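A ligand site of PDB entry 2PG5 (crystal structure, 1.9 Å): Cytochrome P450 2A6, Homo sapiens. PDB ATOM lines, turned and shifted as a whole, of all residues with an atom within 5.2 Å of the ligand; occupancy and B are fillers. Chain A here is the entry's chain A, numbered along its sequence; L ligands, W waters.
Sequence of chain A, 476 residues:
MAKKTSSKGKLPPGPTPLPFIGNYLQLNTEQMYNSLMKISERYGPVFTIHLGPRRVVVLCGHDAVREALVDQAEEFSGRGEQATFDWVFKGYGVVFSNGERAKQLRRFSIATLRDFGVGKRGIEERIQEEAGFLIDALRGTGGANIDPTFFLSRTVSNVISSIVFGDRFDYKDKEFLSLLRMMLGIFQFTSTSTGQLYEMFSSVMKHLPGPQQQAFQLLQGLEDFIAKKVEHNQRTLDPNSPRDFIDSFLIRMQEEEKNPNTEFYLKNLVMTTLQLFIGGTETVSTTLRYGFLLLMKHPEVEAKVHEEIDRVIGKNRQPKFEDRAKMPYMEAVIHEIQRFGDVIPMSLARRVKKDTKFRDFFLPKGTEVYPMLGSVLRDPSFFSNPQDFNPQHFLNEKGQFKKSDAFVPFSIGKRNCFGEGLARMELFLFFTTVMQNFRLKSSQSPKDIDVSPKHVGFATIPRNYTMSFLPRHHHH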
ATOM      1  N   LEU A  69      29.209  35.247   2.292  1.00  0.00           N
ATOM      2  CA  LEU A  69      28.496  34.951   3.525  1.00  0.00           C
ATOM      3  C   LEU A  69      27.979  36.148   4.323  1.00  0.00           C
ATOM      4  O   LEU A  69      27.073  35.984   5.138  1.00  0.00           O
ATOM      5  CB  LEU A  69      29.354  34.053   4.432  1.00  0.00           C
ATOM      6  CG  LEU A  69      29.365  32.548   4.119  1.00  0.00           C
ATOM      7  CD1 LEU A  69      29.758  32.294   2.669  1.00  0.00           C
ATOM      8  CD2 LEU A  69      30.344  31.827   5.060  1.00  0.00           C
ATOM      9  N   ARG A  79      22.161  25.492   3.732  1.00  0.00           N
ATOM     10  CA  ARG A  79      23.058  24.499   4.330  1.00  0.00           C
ATOM     11  C   ARG A  79      23.403  23.412   3.312  1.00  0.00           C
ATOM     12  O   ARG A  79      22.524  22.749   2.765  1.00  0.00           O
ATOM     13  CB  ARG A  79      22.408  23.846   5.567  1.00  0.00           C
ATOM     14  CG  ARG A  79      23.176  22.633   6.130  1.00  0.00           C
ATOM     15  CD  ARG A  79      24.605  22.972   6.579  1.00  0.00           C
ATOM     16  NE  ARG A  79      24.644  23.798   7.778  1.00  0.00           N
ATOM     17  CZ  ARG A  79      25.560  24.723   8.038  1.00  0.00           C
ATOM     18  NH1 ARG A  79      26.530  24.972   7.165  1.00  0.00           N
ATOM     19  NH2 ARG A  79      25.508  25.428   9.166  1.00  0.00           N
ATOM     20  N   VAL A  94      18.912  20.709  13.666  1.00  0.00           N
ATOM     21  CA  VAL A  94      19.284  22.101  13.425  1.00  0.00           C
ATOM     22  C   VAL A  94      20.471  22.368  12.498  1.00  0.00           C
ATOM     23  O   VAL A  94      20.424  23.273  11.670  1.00  0.00           O
ATOM     24  CB  VAL A  94      19.566  22.823  14.780  1.00  0.00           C
ATOM     25  CG1 VAL A  94      20.865  22.305  15.376  1.00  0.00           C
ATOM     26  CG2 VAL A  94      19.611  24.333  14.588  1.00  0.00           C
ATOM     27  N   VAL A  95      21.533  21.584  12.641  1.00  0.00           N
ATOM     28  CA  VAL A  95      22.732  21.805  11.828  1.00  0.00           C
ATOM     29  C   VAL A  95      22.603  21.503  10.341  1.00  0.00           C
ATOM     30  O   VAL A  95      23.019  22.302   9.502  1.00  0.00           O
ATOM     31  CB  VAL A  95      23.929  20.999  12.384  1.00  0.00           C
ATOM     32  CG1 VAL A  95      25.163  21.288  11.554  1.00  0.00           C
ATOM     33  CG2 VAL A  95      24.172  21.357  13.824  1.00  0.00           C
ATOM     34  N   ARG A 106      16.626  26.407  14.685  1.00  0.00           N
ATOM     35  CA  ARG A 106      17.676  27.319  15.126  1.00  0.00           C
ATOM     36  C   ARG A 106      17.127  28.322  16.153  1.00  0.00           C
ATOM     37  O   ARG A 106      17.738  28.554  17.199  1.00  0.00           O
ATOM     38  CB  ARG A 106      18.290  28.061  13.931  1.00  0.00           C
ATOM     39  CG  ARG A 106      19.424  29.009  14.320  1.00  0.00           C
ATOM     40  CD  ARG A 106      20.176  29.575  13.120  1.00  0.00           C
ATOM     41  NE  ARG A 106      21.033  30.701  13.511  1.00  0.00           N
ATOM     42  CZ  ARG A 106      22.366  30.707  13.473  1.00  0.00           C
ATOM     43  NH1 ARG A 106      23.030  29.646  13.046  1.00  0.00           N
ATOM     44  NH2 ARG A 106      23.029  31.782  13.864  1.00  0.00           N
ATOM     45  N   LEU A 113      18.923  27.338  24.699  1.00  0.00           N
ATOM     46  CA  LEU A 113      20.276  27.334  25.250  1.00  0.00           C
ATOM     47  C   LEU A 113      20.402  28.485  26.251  1.00  0.00           C
ATOM     48  O   LEU A 113      20.971  28.325  27.341  1.00  0.00           O
ATOM     49  CB  LEU A 113      21.299  27.501  24.106  1.00  0.00           C
ATOM     50  CG  LEU A 113      22.238  26.316  23.855  1.00  0.00           C
ATOM     51  CD1 LEU A 113      21.528  24.987  24.034  1.00  0.00           C
ATOM     52  CD2 LEU A 113      22.807  26.440  22.450  1.00  0.00           C
ATOM     53  N   ILE A 160      28.204  21.012  27.745  1.00  0.00           N
ATOM     54  CA  ILE A 160      27.036  20.902  26.876  1.00  0.00           C
ATOM     55  C   ILE A 160      26.116  19.782  27.372  1.00  0.00           C
ATOM     56  O   ILE A 160      24.903  19.832  27.174  1.00  0.00           O
ATOM     57  CB  ILE A 160      27.418  20.677  25.382  1.00  0.00           C
ATOM     58  CG1 ILE A 160      26.157  20.621  24.534  1.00  0.00           C
ATOM     59  CG2 ILE A 160      28.273  19.421  25.223  1.00  0.00           C
ATOM     60  CD1 ILE A 160      25.345  21.897  24.540  1.00  0.00           C
ATOM     61  N   LEU A 276      24.241  18.927  18.784  1.00  0.00           N
ATOM     62  CA  LEU A 276      24.743  19.839  19.806  1.00  0.00           C
ATOM     63  C   LEU A 276      25.745  19.122  20.698  1.00  0.00           C
ATOM     64  O   LEU A 276      26.752  19.696  21.119  1.00  0.00           O
ATOM     65  CB  LEU A 276      23.596  20.403  20.639  1.00  0.00           C
ATOM     66  CG  LEU A 276      22.630  21.398  19.986  1.00  0.00           C
ATOM     67  CD1 LEU A 276      21.477  21.684  20.955  1.00  0.00           C
ATOM     68  CD2 LEU A 276      23.366  22.701  19.636  1.00  0.00           C
ATOM     69  N   GLY A 279      28.748  18.730  18.430  1.00  0.00           N
ATOM     70  CA  GLY A 279      29.224  20.076  18.172  1.00  0.00           C
ATOM     71  C   GLY A 279      29.828  20.735  19.391  1.00  0.00           C
ATOM     72  O   GLY A 279      30.892  21.361  19.323  1.00  0.00           O
ATOM     73  N   GLY A 280      29.173  20.578  20.538  1.00  0.00           N
ATOM     74  CA  GLY A 280      29.666  21.186  21.746  1.00  0.00           C
ATOM     75  C   GLY A 280      30.792  20.436  22.425  1.00  0.00           C
ATOM     76  O   GLY A 280      31.300  20.888  23.451  1.00  0.00           O
ATOM     77  N   THR A 283      34.712  19.996  18.974  1.00  0.00           N
ATOM     78  CA  THR A 283      35.315  21.236  18.499  1.00  0.00           C
ATOM     79  C   THR A 283      36.126  21.910  19.601  1.00  0.00           C
ATOM     80  O   THR A 283      37.306  22.210  19.411  1.00  0.00           O
ATOM     81  CB  THR A 283      34.258  22.224  17.967  1.00  0.00           C
ATOM     82  OG1 THR A 283      33.313  22.528  19.002  1.00  0.00           O
ATOM     83  CG2 THR A 283      33.532  21.625  16.760  1.00  0.00           C
ATOM     84  N   VAL A 284      35.500  22.135  20.758  1.00  0.00           N
ATOM     85  CA  VAL A 284      36.199  22.776  21.871  1.00  0.00           C
ATOM     86  C   VAL A 284      37.370  21.902  22.323  1.00  0.00           C
ATOM     87  O   VAL A 284      38.479  22.397  22.548  1.00  0.00           O
ATOM     88  CB  VAL A 284      35.258  23.002  23.075  1.00  0.00           C
ATOM     89  CG1 VAL A 284      36.017  23.697  24.193  1.00  0.00           C
ATOM     90  CG2 VAL A 284      34.058  23.824  22.646  1.00  0.00           C
ATOM     91  N   THR A 287      40.376  21.996  20.076  1.00  0.00           N
ATOM     92  CA  THR A 287      41.030  23.284  20.246  1.00  0.00           C
ATOM     93  C   THR A 287      41.908  23.326  21.504  1.00  0.00           C
ATOM     94  O   THR A 287      43.043  23.784  21.455  1.00  0.00           O
ATOM     95  CB  THR A 287      39.995  24.436  20.313  1.00  0.00           C
ATOM     96  OG1 THR A 287      39.177  24.404  19.135  1.00  0.00           O
ATOM     97  CG2 THR A 287      40.690  25.786  20.405  1.00  0.00           C
ATOM     98  N   GLN A 338      43.116  29.436  18.036  1.00  0.00           N
ATOM     99  CA  GLN A 338      42.011  29.138  17.147  1.00  0.00           C
ATOM    100  C   GLN A 338      42.356  29.441  15.691  1.00  0.00           C
ATOM    101  O   GLN A 338      41.894  28.754  14.777  1.00  0.00           O
ATOM    102  CB  GLN A 338      40.771  29.919  17.553  1.00  0.00           C
ATOM    103  CG  GLN A 338      40.053  29.328  18.749  1.00  0.00           C
ATOM    104  CD  GLN A 338      38.642  29.879  18.890  1.00  0.00           C
ATOM    105  OE1 GLN A 338      38.437  30.963  19.427  1.00  0.00           O
ATOM    106  NE2 GLN A 338      37.668  29.120  18.409  1.00  0.00           N
ATOM    107  N   VAL A 343      40.489  24.543  13.200  1.00  0.00           N
ATOM    108  CA  VAL A 343      39.754  23.307  13.484  1.00  0.00           C
ATOM    109  C   VAL A 343      38.779  22.813  12.400  1.00  0.00           C
ATOM    110  O   VAL A 343      38.733  21.612  12.111  1.00  0.00           O
ATOM    111  CB  VAL A 343      39.033  23.424  14.847  1.00  0.00           C
ATOM    112  CG1 VAL A 343      38.462  22.084  15.260  1.00  0.00           C
ATOM    113  CG2 VAL A 343      40.028  23.926  15.906  1.00  0.00           C
ATOM    114  N   ILE A 344      37.993  23.730  11.820  1.00  0.00           N
ATOM    115  CA  ILE A 344      37.044  23.371  10.773  1.00  0.00           C
ATOM    116  C   ILE A 344      37.518  24.169   9.556  1.00  0.00           C
ATOM    117  O   ILE A 344      36.925  25.182   9.189  1.00  0.00           O
ATOM    118  CB  ILE A 344      35.610  23.798  11.139  1.00  0.00           C
ATOM    119  CG1 ILE A 344      35.261  23.291  12.546  1.00  0.00           C
ATOM    120  CG2 ILE A 344      34.620  23.252  10.118  1.00  0.00           C
ATOM    121  CD1 ILE A 344      35.353  21.782  12.719  1.00  0.00           C
ATOM    122  N   SER A 347      34.923  24.962   6.862  1.00  0.00           N
ATOM    123  CA  SER A 347      33.629  25.264   7.469  1.00  0.00           C
ATOM    124  C   SER A 347      32.664  24.109   7.234  1.00  0.00           C
ATOM    125  O   SER A 347      33.078  22.981   7.014  1.00  0.00           O
ATOM    126  CB  SER A 347      33.050  26.550   6.860  1.00  0.00           C
ATOM    127  OG  SER A 347      32.002  27.083   7.644  1.00  0.00           O
ATOM    128  N   LEU A 348      31.379  24.420   7.293  1.00  0.00           N
ATOM    129  CA  LEU A 348      30.337  23.441   7.042  1.00  0.00           C
ATOM    130  C   LEU A 348      29.704  23.991   5.771  1.00  0.00           C
ATOM    131  O   LEU A 348      29.289  25.159   5.733  1.00  0.00           O
ATOM    132  CB  LEU A 348      29.327  23.432   8.191  1.00  0.00           C
ATOM    133  CG  LEU A 348      28.438  22.204   8.305  1.00  0.00           C
ATOM    134  CD1 LEU A 348      29.295  20.945   8.410  1.00  0.00           C
ATOM    135  CD2 LEU A 348      27.544  22.336   9.520  1.00  0.00           C
ATOM    136  N   ARG A 350      27.752  25.470   2.624  1.00  0.00           N
ATOM    137  CA  ARG A 350      26.567  26.298   2.509  1.00  0.00           C
ATOM    138  C   ARG A 350      26.046  25.968   1.116  1.00  0.00           C
ATOM    139  O   ARG A 350      26.600  25.107   0.434  1.00  0.00           O
ATOM    140  CB  ARG A 350      26.922  27.797   2.538  1.00  0.00           C
ATOM    141  CG  ARG A 350      27.420  28.364   3.876  1.00  0.00           C
ATOM    142  CD  ARG A 350      26.320  28.369   4.912  1.00  0.00           C
ATOM    143  NE  ARG A 350      26.682  29.113   6.104  1.00  0.00           N
ATOM    144  CZ  ARG A 350      26.549  30.438   6.245  1.00  0.00           C
ATOM    145  NH1 ARG A 350      26.043  31.158   5.249  1.00  0.00           N
ATOM    146  NH2 ARG A 350      26.911  31.025   7.367  1.00  0.00           N
ATOM    147  N   LEU A 373      37.429  28.712   5.357  1.00  0.00           N
ATOM    148  CA  LEU A 373      37.808  29.455   6.552  1.00  0.00           C
ATOM    149  C   LEU A 373      39.314  29.459   6.810  1.00  0.00           C
ATOM    150  O   LEU A 373      39.876  30.468   7.232  1.00  0.00           O
ATOM    151  CB  LEU A 373      37.070  28.879   7.781  1.00  0.00           C
ATOM    152  CG  LEU A 373      35.546  28.866   7.706  1.00  0.00           C
ATOM    153  CD1 LEU A 373      34.965  28.288   8.986  1.00  0.00           C
ATOM    154  CD2 LEU A 373      35.030  30.292   7.504  1.00  0.00           C
ATOM    155  N   PRO A 409      36.932  31.563  12.860  1.00  0.00           N
ATOM    156  CA  PRO A 409      36.870  30.124  13.121  1.00  0.00           C
ATOM    157  C   PRO A 409      35.456  29.600  13.334  1.00  0.00           C
ATOM    158  O   PRO A 409      35.204  28.412  13.158  1.00  0.00           O
ATOM    159  CB  PRO A 409      37.735  29.970  14.368  1.00  0.00           C
ATOM    160  CG  PRO A 409      37.442  31.228  15.114  1.00  0.00           C
ATOM    161  CD  PRO A 409      37.466  32.289  14.017  1.00  0.00           C
ATOM    162  N   PHE A 410      34.546  30.502  13.701  1.00  0.00           N
ATOM    163  CA  PHE A 410      33.144  30.146  13.930  1.00  0.00           C
ATOM    164  C   PHE A 410      32.337  30.526  12.688  1.00  0.00           C
ATOM    165  O   PHE A 410      31.107  30.514  12.693  1.00  0.00           O
ATOM    166  CB  PHE A 410      32.589  30.908  15.145  1.00  0.00           C
ATOM    167  CG  PHE A 410      33.294  30.580  16.436  1.00  0.00           C
ATOM    168  CD1 PHE A 410      32.981  29.412  17.144  1.00  0.00           C
ATOM    169  CD2 PHE A 410      34.263  31.431  16.942  1.00  0.00           C
ATOM    170  CE1 PHE A 410      33.629  29.106  18.337  1.00  0.00           C
ATOM    171  CE2 PHE A 410      34.928  31.133  18.148  1.00  0.00           C
ATOM    172  CZ  PHE A 410      34.605  29.962  18.838  1.00  0.00           C
ATOM    173  N   SER A 411      33.049  30.844  11.614  1.00  0.00           N
ATOM    174  CA  SER A 411      32.443  31.258  10.359  1.00  0.00           C
ATOM    175  C   SER A 411      31.664  32.564  10.585  1.00  0.00           C
ATOM    176  O   SER A 411      31.741  33.172  11.666  1.00  0.00           O
ATOM    177  CB  SER A 411      31.505  30.171   9.835  1.00  0.00           C
ATOM    178  OG  SER A 411      31.142  30.421   8.480  1.00  0.00           O
ATOM    179  N   ILE A 412      30.924  32.996   9.575  1.00  0.00           N
ATOM    180  CA  ILE A 412      30.160  34.239   9.651  1.00  0.00           C
ATOM    181  C   ILE A 412      28.860  34.116   8.857  1.00  0.00           C
ATOM    182  O   ILE A 412      28.655  33.137   8.141  1.00  0.00           O
ATOM    183  CB  ILE A 412      30.985  35.396   9.087  1.00  0.00           C
ATOM    184  CG1 ILE A 412      31.489  35.035   7.683  1.00  0.00           C
ATOM    185  CG2 ILE A 412      32.156  35.695  10.008  1.00  0.00           C
ATOM    186  CD1 ILE A 412      32.382  36.073   7.041  1.00  0.00           C
ATOM    187  N   LYS A 414      24.494  34.194   8.250  1.00  0.00           N
ATOM    188  CA  LYS A 414      23.235  33.632   8.752  1.00  0.00           C
ATOM    189  C   LYS A 414      23.230  32.264   9.432  1.00  0.00           C
ATOM    190  O   LYS A 414      22.453  32.040  10.356  1.00  0.00           O
ATOM    191  CB  LYS A 414      22.215  33.599   7.606  1.00  0.00           C
ATOM    192  CG  LYS A 414      21.850  34.949   7.042  1.00  0.00           C
ATOM    193  CD  LYS A 414      21.173  35.815   8.102  1.00  0.00           C
ATOM    194  CE  LYS A 414      20.513  37.046   7.477  1.00  0.00           C
ATOM    195  NZ  LYS A 414      19.428  36.641   6.523  1.00  0.00           N
ATOM    196  N   ARG A 415      24.058  31.343   8.964  1.00  0.00           N
ATOM    197  CA  ARG A 415      24.109  30.018   9.583  1.00  0.00           C
ATOM    198  C   ARG A 415      25.417  29.853  10.344  1.00  0.00           C
ATOM    199  O   ARG A 415      25.931  28.749  10.456  1.00  0.00           O
ATOM    200  CB  ARG A 415      23.970  28.922   8.524  1.00  0.00           C
ATOM    201  CG  ARG A 415      22.617  28.890   7.816  1.00  0.00           C
ATOM    202  CD  ARG A 415      21.513  28.385   8.731  1.00  0.00           C
ATOM    203  NE  ARG A 415      21.677  26.987   9.114  1.00  0.00           N
ATOM    204  CZ  ARG A 415      21.184  25.952   8.450  1.00  0.00           C
ATOM    205  NH1 ARG A 415      21.402  24.718   8.883  1.00  0.00           N
ATOM    206  NH2 ARG A 415      20.454  26.137   7.354  1.00  0.00           N
ATOM    207  N   ASN A 416      25.941  30.957  10.877  1.00  0.00           N
ATOM    208  CA  ASN A 416      27.186  30.925  11.631  1.00  0.00           C
ATOM    209  C   ASN A 416      26.961  30.136  12.916  1.00  0.00           C
ATOM    210  O   ASN A 416      25.828  29.892  13.314  1.00  0.00           O
ATOM    211  CB  ASN A 416      27.659  32.347  11.951  1.00  0.00           C
ATOM    212  CG  ASN A 416      26.781  33.040  12.975  1.00  0.00           C
ATOM    213  OD1 ASN A 416      25.568  32.844  13.008  1.00  0.00           O
ATOM    214  ND2 ASN A 416      27.396  33.881  13.806  1.00  0.00           N
ATOM    215  N   CYS A 417      28.051  29.734  13.555  1.00  0.00           N
ATOM    216  CA  CYS A 417      27.988  28.947  14.795  1.00  0.00           C
ATOM    217  C   CYS A 417      27.290  29.677  15.933  1.00  0.00           C
ATOM    218  O   CYS A 417      27.757  30.711  16.380  1.00  0.00           O
ATOM    219  CB  CYS A 417      29.407  28.580  15.235  1.00  0.00           C
ATOM    220  SG  CYS A 417      29.505  27.599  16.747  1.00  0.00           S
ATOM    221  N   PHE A 418      26.162  29.162  16.424  1.00  0.00           N
ATOM    222  CA  PHE A 418      25.525  29.859  17.520  1.00  0.00           C
ATOM    223  C   PHE A 418      26.008  29.319  18.873  1.00  0.00           C
ATOM    224  O   PHE A 418      25.488  29.670  19.930  1.00  0.00           O
ATOM    225  CB  PHE A 418      23.991  29.851  17.393  1.00  0.00           C
ATOM    226  CG  PHE A 418      23.343  28.499  17.391  1.00  0.00           C
ATOM    227  CD1 PHE A 418      23.246  27.758  18.552  1.00  0.00           C
ATOM    228  CD2 PHE A 418      22.722  28.025  16.235  1.00  0.00           C
ATOM    229  CE1 PHE A 418      22.531  26.553  18.577  1.00  0.00           C
ATOM    230  CE2 PHE A 418      22.005  26.823  16.238  1.00  0.00           C
ATOM    231  CZ  PHE A 418      21.899  26.094  17.425  1.00  0.00           C
ATOM    232  N   GLY A 419      27.053  28.499  18.811  1.00  0.00           N
ATOM    233  CA  GLY A 419      27.653  27.954  20.019  1.00  0.00           C
ATOM    234  C   GLY A 419      28.882  28.762  20.387  1.00  0.00           C
ATOM    235  O   GLY A 419      29.531  28.525  21.408  1.00  0.00           O
ATOM    236  N   GLU A 420      29.203  29.746  19.540  1.00  0.00           N
ATOM    237  CA  GLU A 420      30.359  30.603  19.756  1.00  0.00           C
ATOM    238  C   GLU A 420      30.454  31.189  21.166  1.00  0.00           C
ATOM    239  O   GLU A 420      31.505  31.163  21.796  1.00  0.00           O
ATOM    240  CB  GLU A 420      30.379  31.733  18.722  1.00  0.00           C
ATOM    241  CG  GLU A 420      31.469  32.769  18.985  1.00  0.00           C
ATOM    242  CD  GLU A 420      31.603  33.798  17.878  1.00  0.00           C
ATOM    243  OE1 GLU A 420      32.402  34.738  18.051  1.00  0.00           O
ATOM    244  OE2 GLU A 420      30.915  33.674  16.837  1.00  0.00           O
ATOM    245  N   LEU A 422      29.173  30.107  24.046  1.00  0.00           N
ATOM    246  CA  LEU A 422      29.525  29.032  24.970  1.00  0.00           C
ATOM    247  C   LEU A 422      30.973  28.620  24.777  1.00  0.00           C
ATOM    248  O   LEU A 422      31.736  28.530  25.738  1.00  0.00           O
ATOM    249  CB  LEU A 422      28.613  27.810  24.749  1.00  0.00           C
ATOM    250  CG  LEU A 422      28.854  26.582  25.619  1.00  0.00           C
ATOM    251  CD1 LEU A 422      28.673  26.932  27.087  1.00  0.00           C
ATOM    252  CD2 LEU A 422      27.900  25.476  25.221  1.00  0.00           C
ATOM    253  N   ALA A 423      31.355  28.396  23.525  1.00  0.00           N
ATOM    254  CA  ALA A 423      32.716  27.985  23.185  1.00  0.00           C
ATOM    255  C   ALA A 423      33.763  28.945  23.725  1.00  0.00           C
ATOM    256  O   ALA A 423      34.737  28.527  24.349  1.00  0.00           O
ATOM    257  CB  ALA A 423      32.849  27.862  21.676  1.00  0.00           C
ATOM    258  N   GLU A 426      34.104  28.729  27.449  1.00  0.00           N
ATOM    259  CA  GLU A 426      34.822  27.509  27.799  1.00  0.00           C
ATOM    260  C   GLU A 426      36.315  27.623  27.541  1.00  0.00           C
ATOM    261  O   GLU A 426      37.124  27.275  28.409  1.00  0.00           O
ATOM    262  CB  GLU A 426      34.261  26.319  27.010  1.00  0.00           C
ATOM    263  CG  GLU A 426      32.900  25.867  27.484  1.00  0.00           C
ATOM    264  CD  GLU A 426      32.468  24.539  26.862  1.00  0.00           C
ATOM    265  OE1 GLU A 426      33.329  23.650  26.705  1.00  0.00           O
ATOM    266  OE2 GLU A 426      31.264  24.398  26.560  1.00  0.00           O
ATOM    267  N   LEU A 427      36.693  28.104  26.365  1.00  0.00           N
ATOM    268  CA  LEU A 427      38.106  28.235  26.012  1.00  0.00           C
ATOM    269  C   LEU A 427      38.843  29.124  26.998  1.00  0.00           C
ATOM    270  O   LEU A 427      39.956  28.837  27.400  1.00  0.00           O
ATOM    271  CB  LEU A 427      38.267  28.788  24.588  1.00  0.00           C
ATOM    272  CG  LEU A 427      37.808  27.904  23.423  1.00  0.00           C
ATOM    273  CD1 LEU A 427      38.046  28.613  22.096  1.00  0.00           C
ATOM    274  CD2 LEU A 427      38.560  26.575  23.458  1.00  0.00           C
HETATM  275  C1  LIG L   1      28.073  25.638  13.255  1.00  0.00           C
HETATM  276  C2  LIG L   1      32.671  26.020  14.429  1.00  0.00           C
HETATM  277  C3  LIG L   1      31.569  25.176  18.940  1.00  0.00           C
HETATM  278  C4  LIG L   1      27.064  24.548  17.714  1.00  0.00           C
HETATM  279  C5  LIG L   1      29.459  25.836  13.103  1.00  0.00           C
HETATM  280  C6  LIG L   1      30.144  26.173  11.927  1.00  0.00           C
HETATM  281  C7  LIG L   1      31.479  26.257  12.280  1.00  0.00           C
HETATM  282  C8  LIG L   1      31.535  25.960  13.650  1.00  0.00           C
HETATM  283  C9  LIG L   1      32.705  26.614  11.353  1.00  0.00           C
HETATM  284  C10 LIG L   1      29.503  26.417  10.554  1.00  0.00           C
HETATM  285  C11 LIG L   1      29.099  27.840  10.335  1.00  0.00           C
HETATM  286  C12 LIG L   1      28.495  28.179   8.986  1.00  0.00           C
HETATM  287  O1  LIG L   1      28.681  29.294   8.530  1.00  0.00           O
HETATM  288  O2  LIG L   1      27.847  27.367   8.343  1.00  0.00           O
HETATM  289  C13 LIG L   1      32.863  25.894  15.804  1.00  0.00           C
HETATM  290  C14 LIG L   1      34.106  25.948  16.512  1.00  0.00           C
HETATM  291  C15 LIG L   1      33.758  25.646  17.854  1.00  0.00           C
HETATM  292  C16 LIG L   1      32.359  25.445  17.829  1.00  0.00           C
HETATM  293  C17 LIG L   1      35.451  26.264  15.882  1.00  0.00           C
HETATM  294  C18 LIG L   1      34.583  25.551  19.011  1.00  0.00           C
HETATM  295  C19 LIG L   1      35.906  26.135  19.335  1.00  0.00           C
HETATM  296  C20 LIG L   1      30.211  25.038  19.079  1.00  0.00           C
HETATM  297  C21 LIG L   1      29.572  24.730  20.272  1.00  0.00           C
HETATM  298  C22 LIG L   1      28.263  24.396  19.940  1.00  0.00           C
HETATM  299  C23 LIG L   1      28.199  24.535  18.527  1.00  0.00           C
HETATM  300  C24 LIG L   1      30.195  24.758  21.709  1.00  0.00           C
HETATM  301  C25 LIG L   1      27.195  24.005  20.703  1.00  0.00           C
HETATM  302  C26 LIG L   1      26.412  24.762  21.596  1.00  0.00           C
HETATM  303  C27 LIG L   1      26.940  24.712  16.378  1.00  0.00           C
HETATM  304  C28 LIG L   1      25.748  24.532  15.670  1.00  0.00           C
HETATM  305  C29 LIG L   1      26.011  24.839  14.363  1.00  0.00           C
HETATM  306  C30 LIG L   1      27.375  25.210  14.360  1.00  0.00           C
HETATM  307  C31 LIG L   1      24.381  24.067  16.229  1.00  0.00           C
HETATM  308  C32 LIG L   1      25.023  24.806  13.153  1.00  0.00           C
HETATM  309  C33 LIG L   1      24.294  26.182  12.949  1.00  0.00           C
HETATM  310  C34 LIG L   1      23.270  26.285  11.797  1.00  0.00           C
HETATM  311  O3  LIG L   1      22.467  27.187  11.770  1.00  0.00           O
HETATM  312  O4  LIG L   1      23.255  25.421  10.913  1.00  0.00           O
HETATM  313  N1  LIG L   1      30.345  25.715  14.138  1.00  0.00           N
HETATM  314  N2  LIG L   1      31.863  25.601  16.619  1.00  0.00           N
HETATM  315  N3  LIG L   1      29.394  24.918  18.051  1.00  0.00           N
HETATM  316  N4  LIG L   1      27.883  25.108  15.591  1.00  0.00           N
HETATM  317 FE1  LIG L   1      29.870  25.386  16.119  1.00  0.00          FE
HETATM  318  O   HOH W   1      29.834  27.985   6.161  1.00  0.00           O
HETATM  319  O   HOH W   2      29.809  22.830  15.742  1.00  0.00           O
HETATM  320  O   HOH W   3      19.636  26.140  11.599  1.00  0.00           O
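O1 of the ligand lies within salt-bridge range of NH2 of Arg 350 (2.7 Å). The guanidinium group (NE) of Arg 415 lies within salt-bridge range of an oxygen (O3) of the ligand (2.8 Å). OG of Ser 411 lies within hydrogen-bond range of O1 of the ligand (2.7 Å). The guanidinium group (NH1) of Arg 106 lies within salt-bridge range of an oxygen (O3) of the ligand, 2.8 Å away. An iron atom (FE1) of the ligand is bound by the side-chain sulfur (SG) of Cys 417, 2.3 Å away. NH2 of Arg 79 is in salt-bridge range of O4 of the ligand, 2.9 Å away.
O of Ile 412 is in hydrogen-bond range of NH2 of Arg 350 (2.8 Å). The backbone carbonyl oxygen (O) of Thr 283 lies within hydrogen-bond range of the side-chain hydroxyl (OG1) of Thr 287, at 2.9 Å. O of Gly 279 lies within hydrogen-bond range of OG1 of Thr 283, 2.7 Å away. The side-chain sulfur of Cys 417 lies close to the backbone NH of Gly 419, at 3.3 Å. The backbone NH (N) of Cys 417 sits at hydrogen-bond distance from the backbone carbonyl oxygen (O) of Phe 410 (3.3 Å). The guanidinium group of Arg 79 lies within hydrogen-bond range of the backbone carbonyl oxygen of Leu 348, 3.1 Å away. The guanidinium group of Arg 415 lies within hydrogen-bond range of the backbone carbonyl oxygen of Val 94, 3.3 Å away. The guanidinium group of Arg 106 lies within hydrogen-bond range of the backbone carbonyl oxygen of Asn 416 (2.8 Å).
An oxygen (O4) of the ligand lies close to the backbone carbonyl oxygen of Val 95 (3.4 Å). Residues that only touch the ligand: Thr 283 (3.2 Å), Phe 418 (3.4 Å), Pro 409 (3.5 Å), Phe 410 (3.5 Å), Gln 338 (3.6 Å), Gly 419 (3.6 Å), Gly 280 (3.6 Å), Val 94 (3.6 Å), Leu 373 (3.7 Å), Thr 287 (3.7 Å), Leu 348 (3.7 Å), Gly 279 (3.7 Å), Ser 347 (3.8 Å), Leu 276 (3.8 Å), Asn 416 (3.8 Å), Ile 412 (3.9 Å), Ala 423 (3.9 Å), Val 284 (3.9 Å) and Leu 422 (3.98 Å). Hydrophobic or aromatic side chains within 4 Å of the ligand: Val 95, Leu 276, Leu 348, Leu 373, Phe 410, Phe 418, Leu 422 and Ala 423.
Water W1 lies within hydrogen-bond range of OG of Ser 347 (2.8 Å), O of Leu 348 (2.9 Å), O1 of the ligand (2.9 Å) and NE of Arg 350 (3.3 Å). Water W3 lies within hydrogen-bond range of O of Val 94, O3 of the ligand and NE of Arg 415.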
